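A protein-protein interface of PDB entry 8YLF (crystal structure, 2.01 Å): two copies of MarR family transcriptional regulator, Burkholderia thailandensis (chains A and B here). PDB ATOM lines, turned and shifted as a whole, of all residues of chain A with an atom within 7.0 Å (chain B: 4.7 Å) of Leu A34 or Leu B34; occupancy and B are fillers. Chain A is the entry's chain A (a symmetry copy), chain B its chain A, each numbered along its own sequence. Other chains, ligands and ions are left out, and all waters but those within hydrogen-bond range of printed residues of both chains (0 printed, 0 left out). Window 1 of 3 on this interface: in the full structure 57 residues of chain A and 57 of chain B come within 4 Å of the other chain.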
ATOM      1  N   MET A  28      30.808 -21.421  -9.629  1.00  0.00           N
ATOM      2  CA  MET A  28      29.504 -21.987  -9.289  1.00  0.00           C
ATOM      3  C   MET A  28      29.003 -21.503  -7.934  1.00  0.00           C
ATOM      4  O   MET A  28      27.788 -21.455  -7.713  1.00  0.00           O
ATOM      5  CB  MET A  28      29.566 -23.513  -9.284  1.00  0.00           C
ATOM      6  CG  MET A  28      29.671 -24.141 -10.645  1.00  0.00           C
ATOM      7  SD  MET A  28      29.611 -25.934 -10.486  1.00  0.00           S
ATOM      8  CE  MET A  28      29.583 -26.427 -12.209  1.00  0.00           C
ATOM      9  N   ILE A  29      29.911 -21.154  -7.020  1.00  0.00           N
ATOM     10  CA  ILE A  29      29.498 -20.749  -5.678  1.00  0.00           C
ATOM     11  C   ILE A  29      28.702 -19.454  -5.735  1.00  0.00           C
ATOM     12  O   ILE A  29      27.546 -19.395  -5.300  1.00  0.00           O
ATOM     13  CB  ILE A  29      30.718 -20.603  -4.753  1.00  0.00           C
ATOM     14  CG1 ILE A  29      31.495 -21.918  -4.688  1.00  0.00           C
ATOM     15  CG2 ILE A  29      30.281 -20.148  -3.360  1.00  0.00           C
ATOM     16  CD1 ILE A  29      31.121 -22.773  -3.552  1.00  0.00           C
ATOM     17  N   VAL A  30      29.311 -18.396  -6.278  1.00  0.00           N
ATOM     18  CA  VAL A  30      28.674 -17.083  -6.258  1.00  0.00           C
ATOM     19  C   VAL A  30      27.399 -17.088  -7.099  1.00  0.00           C
ATOM     20  O   VAL A  30      26.357 -16.578  -6.665  1.00  0.00           O
ATOM     21  CB  VAL A  30      29.675 -15.992  -6.703  1.00  0.00           C
ATOM     22  CG1 VAL A  30      30.289 -16.321  -8.054  1.00  0.00           C
ATOM     23  CG2 VAL A  30      29.028 -14.609  -6.726  1.00  0.00           C
ATOM     24  N   LEU A  31      27.438 -17.696  -8.292  1.00  0.00           N
ATOM     25  CA  LEU A  31      26.256 -17.649  -9.147  1.00  0.00           C
ATOM     26  C   LEU A  31      25.181 -18.632  -8.682  1.00  0.00           C
ATOM     27  O   LEU A  31      23.985 -18.353  -8.838  1.00  0.00           O
ATOM     28  CB  LEU A  31      26.636 -17.909 -10.611  1.00  0.00           C
ATOM     29  CG  LEU A  31      27.449 -16.836 -11.353  1.00  0.00           C
ATOM     30  CD1 LEU A  31      27.651 -17.191 -12.826  1.00  0.00           C
ATOM     31  CD2 LEU A  31      26.795 -15.464 -11.230  1.00  0.00           C
ATOM     32  N   GLY A  32      25.577 -19.772  -8.105  1.00  0.00           N
ATOM     33  CA  GLY A  32      24.592 -20.660  -7.504  1.00  0.00           C
ATOM     34  C   GLY A  32      23.908 -20.025  -6.306  1.00  0.00           C
ATOM     35  O   GLY A  32      22.689 -20.139  -6.144  1.00  0.00           O
ATOM     36  N   ARG A  33      24.681 -19.337  -5.456  1.00  0.00           N
ATOM     37  CA  ARG A  33      24.070 -18.639  -4.327  1.00  0.00           C
ATOM     38  C   ARG A  33      23.227 -17.461  -4.786  1.00  0.00           C
ATOM     39  O   ARG A  33      22.192 -17.172  -4.174  1.00  0.00           O
ATOM     40  CB  ARG A  33      25.134 -18.161  -3.345  1.00  0.00           C
ATOM     41  CG  ARG A  33      25.636 -19.263  -2.459  1.00  0.00           C
ATOM     42  CD  ARG A  33      26.704 -18.784  -1.507  1.00  0.00           C
ATOM     43  NE  ARG A  33      27.361 -19.948  -0.941  1.00  0.00           N
ATOM     44  CZ  ARG A  33      28.562 -19.935  -0.384  1.00  0.00           C
ATOM     45  NH1 ARG A  33      29.254 -18.800  -0.305  1.00  0.00           N
ATOM     46  NH2 ARG A  33      29.063 -21.070   0.085  1.00  0.00           N
ATOM     47  N   LEU A  34      23.656 -16.770  -5.848  1.00  0.00           N
ATOM     48  CA  LEU A  34      22.866 -15.662  -6.379  1.00  0.00           C
ATOM     49  C   LEU A  34      21.489 -16.138  -6.811  1.00  0.00           C
ATOM     50  O   LEU A  34      20.466 -15.548  -6.440  1.00  0.00           O
ATOM     51  CB  LEU A  34      23.594 -15.007  -7.557  1.00  0.00           C
ATOM     52  CG  LEU A  34      22.799 -13.939  -8.317  1.00  0.00           C
ATOM     53  CD1 LEU A  34      22.767 -12.654  -7.511  1.00  0.00           C
ATOM     54  CD2 LEU A  34      23.415 -13.664  -9.686  1.00  0.00           C
ATOM     55  N   GLN A  35      21.441 -17.200  -7.617  1.00  0.00           N
ATOM     56  CA  GLN A  35      20.150 -17.644  -8.138  1.00  0.00           C
ATOM     57  C   GLN A  35      19.312 -18.295  -7.043  1.00  0.00           C
ATOM     58  O   GLN A  35      18.085 -18.134  -7.008  1.00  0.00           O
ATOM     59  CB  GLN A  35      20.361 -18.594  -9.321  1.00  0.00           C
ATOM     60  CG  GLN A  35      21.249 -17.991 -10.432  1.00  0.00           C
ATOM     61  CD  GLN A  35      21.448 -18.916 -11.634  1.00  0.00           C
ATOM     62  OE1 GLN A  35      20.632 -18.934 -12.556  1.00  0.00           O
ATOM     63  NE2 GLN A  35      22.545 -19.676 -11.630  1.00  0.00           N
ATOM     64  N   GLU A  36      19.945 -19.046  -6.147  1.00  0.00           N
ATOM     65  CA  GLU A  36      19.183 -19.643  -5.050  1.00  0.00           C
ATOM     66  C   GLU A  36      18.623 -18.576  -4.113  1.00  0.00           C
ATOM     67  O   GLU A  36      17.474 -18.683  -3.650  1.00  0.00           O
ATOM     68  CB  GLU A  36      20.057 -20.636  -4.280  1.00  0.00           C
ATOM     69  CG  GLU A  36      19.339 -21.345  -3.140  1.00  0.00           C
ATOM     70  CD  GLU A  36      18.305 -22.349  -3.628  1.00  0.00           C
ATOM     71  OE1 GLU A  36      18.052 -22.430  -4.858  1.00  0.00           O
ATOM     72  OE2 GLU A  36      17.750 -23.072  -2.768  1.00  0.00           O
ATOM     73  N   ALA A  37      19.412 -17.542  -3.807  1.00  0.00           N
ATOM     74  CA  ALA A  37      18.916 -16.503  -2.910  1.00  0.00           C
ATOM     75  C   ALA A  37      17.756 -15.746  -3.542  1.00  0.00           C
ATOM     76  O   ALA A  37      16.760 -15.461  -2.871  1.00  0.00           O
ATOM     77  CB  ALA A  37      20.043 -15.544  -2.509  1.00  0.00           C
ATOM     78  N   ALA A  38      17.864 -15.408  -4.829  1.00  0.00           N
ATOM     79  CA  ALA A  38      16.763 -14.718  -5.485  1.00  0.00           C
ATOM     80  C   ALA A  38      15.509 -15.577  -5.472  1.00  0.00           C
ATOM     81  O   ALA A  38      14.407 -15.083  -5.204  1.00  0.00           O
ATOM     82  CB  ALA A  38      17.150 -14.346  -6.924  1.00  0.00           C
ATOM     83  N   LEU A  39      15.662 -16.872  -5.748  1.00  0.00           N
ATOM     84  CA  LEU A  39      14.511 -17.768  -5.823  1.00  0.00           C
ATOM     85  C   LEU A  39      13.847 -17.945  -4.459  1.00  0.00           C
ATOM     86  O   LEU A  39      12.620 -17.822  -4.333  1.00  0.00           O
ATOM     87  CB  LEU A  39      14.954 -19.119  -6.391  1.00  0.00           C
ATOM     88  CG  LEU A  39      13.904 -20.228  -6.460  1.00  0.00           C
ATOM     89  CD1 LEU A  39      12.798 -19.852  -7.439  1.00  0.00           C
ATOM     90  CD2 LEU A  39      14.528 -21.590  -6.824  1.00  0.00           C
ATOM     91  N   ILE A  41      14.007 -16.133  -1.728  1.00  0.00           N
ATOM     92  CA  ILE A  41      13.439 -14.894  -1.200  1.00  0.00           C
ATOM     93  C   ILE A  41      12.129 -14.565  -1.905  1.00  0.00           C
ATOM     94  O   ILE A  41      11.130 -14.216  -1.264  1.00  0.00           O
ATOM     95  CB  ILE A  41      14.457 -13.746  -1.312  1.00  0.00           C
ATOM     96  CG1 ILE A  41      15.607 -13.981  -0.321  1.00  0.00           C
ATOM     97  CG2 ILE A  41      13.790 -12.383  -1.050  1.00  0.00           C
ATOM     98  CD1 ILE A  41      16.750 -12.995  -0.461  1.00  0.00           C
ATOM     99  N   ILE A  86      11.903  -4.751 -12.080  1.00  0.00           N
ATOM    100  CA  ILE A  86      12.420  -5.991 -12.651  1.00  0.00           C
ATOM    101  C   ILE A  86      12.043  -6.067 -14.128  1.00  0.00           C
ATOM    102  O   ILE A  86      10.911  -5.752 -14.507  1.00  0.00           O
ATOM    103  CB  ILE A  86      11.873  -7.227 -11.908  1.00  0.00           C
ATOM    104  CG1 ILE A  86      12.024  -7.070 -10.385  1.00  0.00           C
ATOM    105  CG2 ILE A  86      12.587  -8.489 -12.401  1.00  0.00           C
ATOM    106  CD1 ILE A  86      13.455  -7.141  -9.919  1.00  0.00           C
ATOM    107  N   VAL A 142      13.640  -9.529   5.600  1.00  0.00           N
ATOM    108  CA  VAL A 142      14.421 -10.401   4.722  1.00  0.00           C
ATOM    109  C   VAL A 142      15.907 -10.091   4.849  1.00  0.00           C
ATOM    110  O   VAL A 142      16.751 -10.993   4.835  1.00  0.00           O
ATOM    111  CB  VAL A 142      13.946 -10.262   3.261  1.00  0.00           C
ATOM    112  CG1 VAL A 142      14.907 -10.994   2.322  1.00  0.00           C
ATOM    113  CG2 VAL A 142      12.534 -10.800   3.089  1.00  0.00           C
ATOM    114  N   LEU A 143      16.250  -8.811   4.972  1.00  0.00           N
ATOM    115  CA  LEU A 143      17.636  -8.357   4.935  1.00  0.00           C
ATOM    116  C   LEU A 143      18.270  -8.253   6.311  1.00  0.00           C
ATOM    117  O   LEU A 143      19.454  -7.908   6.410  1.00  0.00           O
ATOM    118  CB  LEU A 143      17.714  -6.993   4.252  1.00  0.00           C
ATOM    119  CG  LEU A 143      17.432  -7.045   2.754  1.00  0.00           C
ATOM    120  CD1 LEU A 143      17.031  -5.670   2.270  1.00  0.00           C
ATOM    121  CD2 LEU A 143      18.665  -7.534   2.020  1.00  0.00           C
ATOM    122  N   LEU A 154      26.596  -5.336  -0.424  1.00  0.00           N
ATOM    123  CA  LEU A 154      25.976  -6.268  -1.358  1.00  0.00           C
ATOM    124  C   LEU A 154      25.384  -5.531  -2.553  1.00  0.00           C
ATOM    125  O   LEU A 154      25.473  -6.011  -3.688  1.00  0.00           O
ATOM    126  CB  LEU A 154      24.907  -7.095  -0.640  1.00  0.00           C
ATOM    127  CG  LEU A 154      24.172  -8.183  -1.424  1.00  0.00           C
ATOM    128  CD1 LEU A 154      25.163  -9.107  -2.081  1.00  0.00           C
ATOM    129  CD2 LEU A 154      23.281  -8.981  -0.485  1.00  0.00           C
ATOM    130  N   LEU A 158      26.436  -6.237  -6.493  1.00  0.00           N
ATOM    131  CA  LEU A 158      25.408  -6.583  -7.473  1.00  0.00           C
ATOM    132  C   LEU A 158      25.306  -5.534  -8.572  1.00  0.00           C
ATOM    133  O   LEU A 158      25.028  -5.869  -9.730  1.00  0.00           O
ATOM    134  CB  LEU A 158      24.054  -6.763  -6.778  1.00  0.00           C
ATOM    135  CG  LEU A 158      23.968  -7.991  -5.883  1.00  0.00           C
ATOM    136  CD1 LEU A 158      22.709  -7.942  -5.021  1.00  0.00           C
ATOM    137  CD2 LEU A 158      24.006  -9.264  -6.732  1.00  0.00           C
ATOM    138  N   LEU A 161      28.290  -6.321 -10.920  1.00  0.00           N
ATOM    139  CA  LEU A 161      27.973  -7.526 -11.681  1.00  0.00           C
ATOM    140  C   LEU A 161      26.963  -7.216 -12.778  1.00  0.00           C
ATOM    141  O   LEU A 161      27.129  -7.624 -13.935  1.00  0.00           O
ATOM    142  CB  LEU A 161      27.434  -8.601 -10.739  1.00  0.00           C
ATOM    143  CG  LEU A 161      27.085  -9.972 -11.313  1.00  0.00           C
ATOM    144  CD1 LEU A 161      28.292 -10.600 -11.993  1.00  0.00           C
ATOM    145  CD2 LEU A 161      26.539 -10.892 -10.210  1.00  0.00           C
ATOM    146  N   LEU A 162      25.922  -6.458 -12.430  1.00  0.00           N
ATOM    147  CA  LEU A 162      24.833  -6.179 -13.359  1.00  0.00           C
ATOM    148  C   LEU A 162      25.322  -5.402 -14.573  1.00  0.00           C
ATOM    149  O   LEU A 162      24.979  -5.736 -15.712  1.00  0.00           O
ATOM    150  CB  LEU A 162      23.733  -5.397 -12.642  1.00  0.00           C
ATOM    151  CG  LEU A 162      22.411  -6.062 -12.301  1.00  0.00           C
ATOM    152  CD1 LEU A 162      21.495  -5.021 -11.663  1.00  0.00           C
ATOM    153  CD2 LEU A 162      21.779  -6.638 -13.556  1.00  0.00           C
ATOM    154  N   VAL B  30      19.103  -3.312  -2.761  1.00  0.00           N
ATOM    155  CA  VAL B  30      19.824  -4.581  -2.728  1.00  0.00           C
ATOM    156  C   VAL B  30      18.945  -5.714  -3.254  1.00  0.00           C
ATOM    157  O   VAL B  30      19.396  -6.537  -4.064  1.00  0.00           O
ATOM    158  CB  VAL B  30      20.361  -4.858  -1.304  1.00  0.00           C
ATOM    159  CG1 VAL B  30      19.251  -4.792  -0.269  1.00  0.00           C
ATOM    160  CG2 VAL B  30      21.092  -6.197  -1.230  1.00  0.00           C
ATOM    161  N   LEU B  31      17.669  -5.759  -2.846  1.00  0.00           N
ATOM    162  CA  LEU B  31      16.831  -6.875  -3.274  1.00  0.00           C
ATOM    163  C   LEU B  31      16.363  -6.709  -4.720  1.00  0.00           C
ATOM    164  O   LEU B  31      16.194  -7.708  -5.430  1.00  0.00           O
ATOM    165  CB  LEU B  31      15.633  -7.047  -2.329  1.00  0.00           C
ATOM    166  CG  LEU B  31      15.902  -7.549  -0.902  1.00  0.00           C
ATOM    167  CD1 LEU B  31      14.605  -7.773  -0.124  1.00  0.00           C
ATOM    168  CD2 LEU B  31      16.732  -8.826  -0.912  1.00  0.00           C
ATOM    169  N   GLY B  32      16.155  -5.468  -5.177  1.00  0.00           N
ATOM    170  CA  GLY B  32      15.865  -5.254  -6.587  1.00  0.00           C
ATOM    171  C   GLY B  32      17.040  -5.630  -7.474  1.00  0.00           C
ATOM    172  O   GLY B  32      16.860  -6.255  -8.524  1.00  0.00           O
ATOM    173  N   ARG B  33      18.259  -5.265  -7.058  1.00  0.00           N
ATOM    174  CA  ARG B  33      19.435  -5.665  -7.830  1.00  0.00           C
ATOM    175  C   ARG B  33      19.670  -7.163  -7.756  1.00  0.00           C
ATOM    176  O   ARG B  33      20.118  -7.763  -8.741  1.00  0.00           O
ATOM    177  CB  ARG B  33      20.676  -4.923  -7.347  1.00  0.00           C
ATOM    178  CG  ARG B  33      20.748  -3.518  -7.868  1.00  0.00           C
ATOM    179  CD  ARG B  33      21.969  -2.787  -7.368  1.00  0.00           C
ATOM    180  NE  ARG B  33      21.789  -1.371  -7.631  1.00  0.00           N
ATOM    181  CZ  ARG B  33      22.443  -0.403  -7.010  1.00  0.00           C
ATOM    182  NH1 ARG B  33      23.348  -0.695  -6.075  1.00  0.00           N
ATOM    183  NH2 ARG B  33      22.178   0.857  -7.328  1.00  0.00           N
ATOM    184  N   LEU B  34      19.383  -7.779  -6.605  1.00  0.00           N
ATOM    185  CA  LEU B  34      19.529  -9.227  -6.481  1.00  0.00           C
ATOM    186  C   LEU B  34      18.645  -9.947  -7.485  1.00  0.00           C
ATOM    187  O   LEU B  34      19.103 -10.837  -8.216  1.00  0.00           O
ATOM    188  CB  LEU B  34      19.189  -9.678  -5.058  1.00  0.00           C
ATOM    189  CG  LEU B  34      19.137 -11.193  -4.835  1.00  0.00           C
ATOM    190  CD1 LEU B  34      20.546 -11.750  -4.767  1.00  0.00           C
ATOM    191  CD2 LEU B  34      18.393 -11.536  -3.548  1.00  0.00           C
ATOM    192  N   GLN B  35      17.360  -9.590  -7.526  1.00  0.00           N
ATOM    193  CA  GLN B  35      16.445 -10.313  -8.406  1.00  0.00           C
ATOM    194  C   GLN B  35      16.704  -9.967  -9.869  1.00  0.00           C
ATOM    195  O   GLN B  35      16.600 -10.832 -10.748  1.00  0.00           O
ATOM    196  CB  GLN B  35      14.995 -10.017  -8.010  1.00  0.00           C
ATOM    197  CG  GLN B  35      14.702 -10.305  -6.522  1.00  0.00           C
ATOM    198  CD  GLN B  35      13.252 -10.042  -6.114  1.00  0.00           C
ATOM    199  OE1 GLN B  35      12.390 -10.910  -6.257  1.00  0.00           O
ATOM    200  NE2 GLN B  35      12.984  -8.843  -5.591  1.00  0.00           N
ATOM    201  N   GLU B  36      17.028  -8.710 -10.157  1.00  0.00           N
ATOM    202  CA  GLU B  36      17.337  -8.353 -11.542  1.00  0.00           C
ATOM    203  C   GLU B  36      18.609  -9.043 -12.028  1.00  0.00           C
ATOM    204  O   GLU B  36      18.673  -9.509 -13.177  1.00  0.00           O
ATOM    205  CB  GLU B  36      17.459  -6.833 -11.679  1.00  0.00           C
ATOM    206  CG  GLU B  36      17.739  -6.356 -13.098  1.00  0.00           C
ATOM    207  CD  GLU B  36      16.545  -6.530 -14.025  1.00  0.00           C
ATOM    208  OE1 GLU B  36      15.518  -7.125 -13.607  1.00  0.00           O
ATOM    209  OE2 GLU B  36      16.634  -6.053 -15.180  1.00  0.00           O
ATOM    210  N   ALA B  37      19.639  -9.116 -11.178  1.00  0.00           N
ATOM    211  CA  ALA B  37      20.875  -9.763 -11.605  1.00  0.00           C
ATOM    212  C   ALA B  37      20.655 -11.250 -11.849  1.00  0.00           C
ATOM    213  O   ALA B  37      21.151 -11.799 -12.836  1.00  0.00           O
ATOM    214  CB  ALA B  37      21.991  -9.536 -10.580  1.00  0.00           C
ATOM    215  N   ALA B  38      19.916 -11.921 -10.963  1.00  0.00           N
ATOM    216  CA  ALA B  38      19.647 -13.335 -11.177  1.00  0.00           C
ATOM    217  C   ALA B  38      18.880 -13.544 -12.473  1.00  0.00           C
ATOM    218  O   ALA B  38      19.185 -14.460 -13.246  1.00  0.00           O
ATOM    219  CB  ALA B  38      18.868 -13.916  -9.988  1.00  0.00           C
ATOM    220  N   ILE B  41      21.074 -12.623 -15.777  1.00  0.00           N
ATOM    221  CA  ILE B  41      22.143 -13.597 -15.987  1.00  0.00           C
ATOM    222  C   ILE B  41      21.571 -14.922 -16.476  1.00  0.00           C
ATOM    223  O   ILE B  41      22.086 -15.526 -17.426  1.00  0.00           O
ATOM    224  CB  ILE B  41      22.973 -13.768 -14.702  1.00  0.00           C
ATOM    225  CG1 ILE B  41      23.789 -12.494 -14.445  1.00  0.00           C
ATOM    226  CG2 ILE B  41      23.901 -14.994 -14.799  1.00  0.00           C
ATOM    227  CD1 ILE B  41      24.520 -12.490 -13.115  1.00  0.00           C
ATOM    228  N   LEU B 158      26.039 -13.324   0.033  1.00  0.00           N
ATOM    229  CA  LEU B 158      24.888 -14.130  -0.371  1.00  0.00           C
ATOM    230  C   LEU B 158      24.699 -15.334   0.543  1.00  0.00           C
ATOM    231  O   LEU B 158      23.560 -15.746   0.802  1.00  0.00           O
ATOM    232  CB  LEU B 158      25.044 -14.583  -1.826  1.00  0.00           C
ATOM    233  CG  LEU B 158      24.932 -13.460  -2.848  1.00  0.00           C
ATOM    234  CD1 LEU B 158      25.376 -13.941  -4.227  1.00  0.00           C
ATOM    235  CD2 LEU B 158      23.498 -12.925  -2.885  1.00  0.00           C
ATOM    236  N   LEU B 161      22.994 -13.870   3.703  1.00  0.00           N
ATOM    237  CA  LEU B 161      21.603 -13.568   3.380  1.00  0.00           C
ATOM    238  C   LEU B 161      20.779 -14.847   3.313  1.00  0.00           C
ATOM    239  O   LEU B 161      19.681 -14.932   3.877  1.00  0.00           O
ATOM    240  CB  LEU B 161      21.537 -12.813   2.054  1.00  0.00           C
ATOM    241  CG  LEU B 161      20.176 -12.345   1.541  1.00  0.00           C
ATOM    242  CD1 LEU B 161      19.495 -11.439   2.556  1.00  0.00           C
ATOM    243  CD2 LEU B 161      20.327 -11.634   0.189  1.00  0.00           C
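Of the 12 printed residues of chain B, 12 touch a printed residue of chain A. Printed residues of chain B that touch a printed residue of chain A: Val B30, Leu B31, Gly B32, Arg B33, Leu B34, Gln B35, Glu B36, Ala B37, Ala B38, Ile B41, Leu B158 and Leu B161. Of the 20 printed residues of chain A, 12 touch a printed residue of chain B. Hydrophobic or aromatic side chains of chain A within 4 Å of the printed part of chain B: Leu A34, Ala A38, Ile A41, Ile A86, Leu A143, Leu A154, Leu A158, Leu A161 and Leu A162. Among the printed residues, no Asp or Glu carboxylate lies within 4 Å of a Lys or Arg side-chain nitrogen of the other chain.
Val A30 touches Leu B158, and with the chains exchanged Leu A158 touches Val B30. Arg A33 touches Leu B158, and with the chains exchanged Leu A158 touches Arg B33. Leu A34 touches Ile B41, and with the chains exchanged Ile A41 touches Leu B34. Ile A41 touches Leu B161, and with the chains exchanged Leu A161 touches Ile B41. Of the 20 pairs that touch across the chains among the printed residues, 12 have their exchanged pair printed and touching as well.
The side-chain amide nitrogen of Gln B35 sits close to the backbone carbonyl oxygen of Leu B31 (3.4 Å).
Ile A29 touches none of the printed residues of chain B. Leu A34 touches just these residues of chain B: Leu B34 (3.6 Å), Ile B41 (3.8 Å) and Leu B158 (3.7 Å). Ala A37 touches none of the printed residues of chain B. Of the printed residues of chain B, Val A142 touches Leu B161. Of the printed residues of chain B, Leu A161 touches Ile B41 (3.9 Å). Printed residues of chain B within 4 Å of Leu A162: Ala B37 (3.8 Å). Of the printed residues of chain A, Leu B158 touches Val A30 (3.7 Å), Arg A33 (3.9 Å) and Leu A34 (3.7 Å). The nearest residue of chain A that does not touch Leu B34 is Ala A38 (4.1 Å).
Among the printed residues, pairs that only touch across the chains: Val A30 with Leu B158, Arg A33 with Leu B158, Leu A34 with Leu B34, Leu A34 with Ile B41, Leu A34 with Leu B158, Ala A38 with Ala B38, Ile A41 with Leu B34, Ile A41 with Leu B161, Ile A86 with Gly B32, Ile A86 with Gln B35, Ile A86 with Glu B36, Val A142 with Leu B161, Leu A143 with Val B30, Leu A143 with Leu B31, Leu A154 with Val B30, Leu A158 with Val B30, Leu A158 with Arg B33, Leu A158 with Leu B34, Leu A161 with Ile B41 and Leu A162 with Ala B37.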
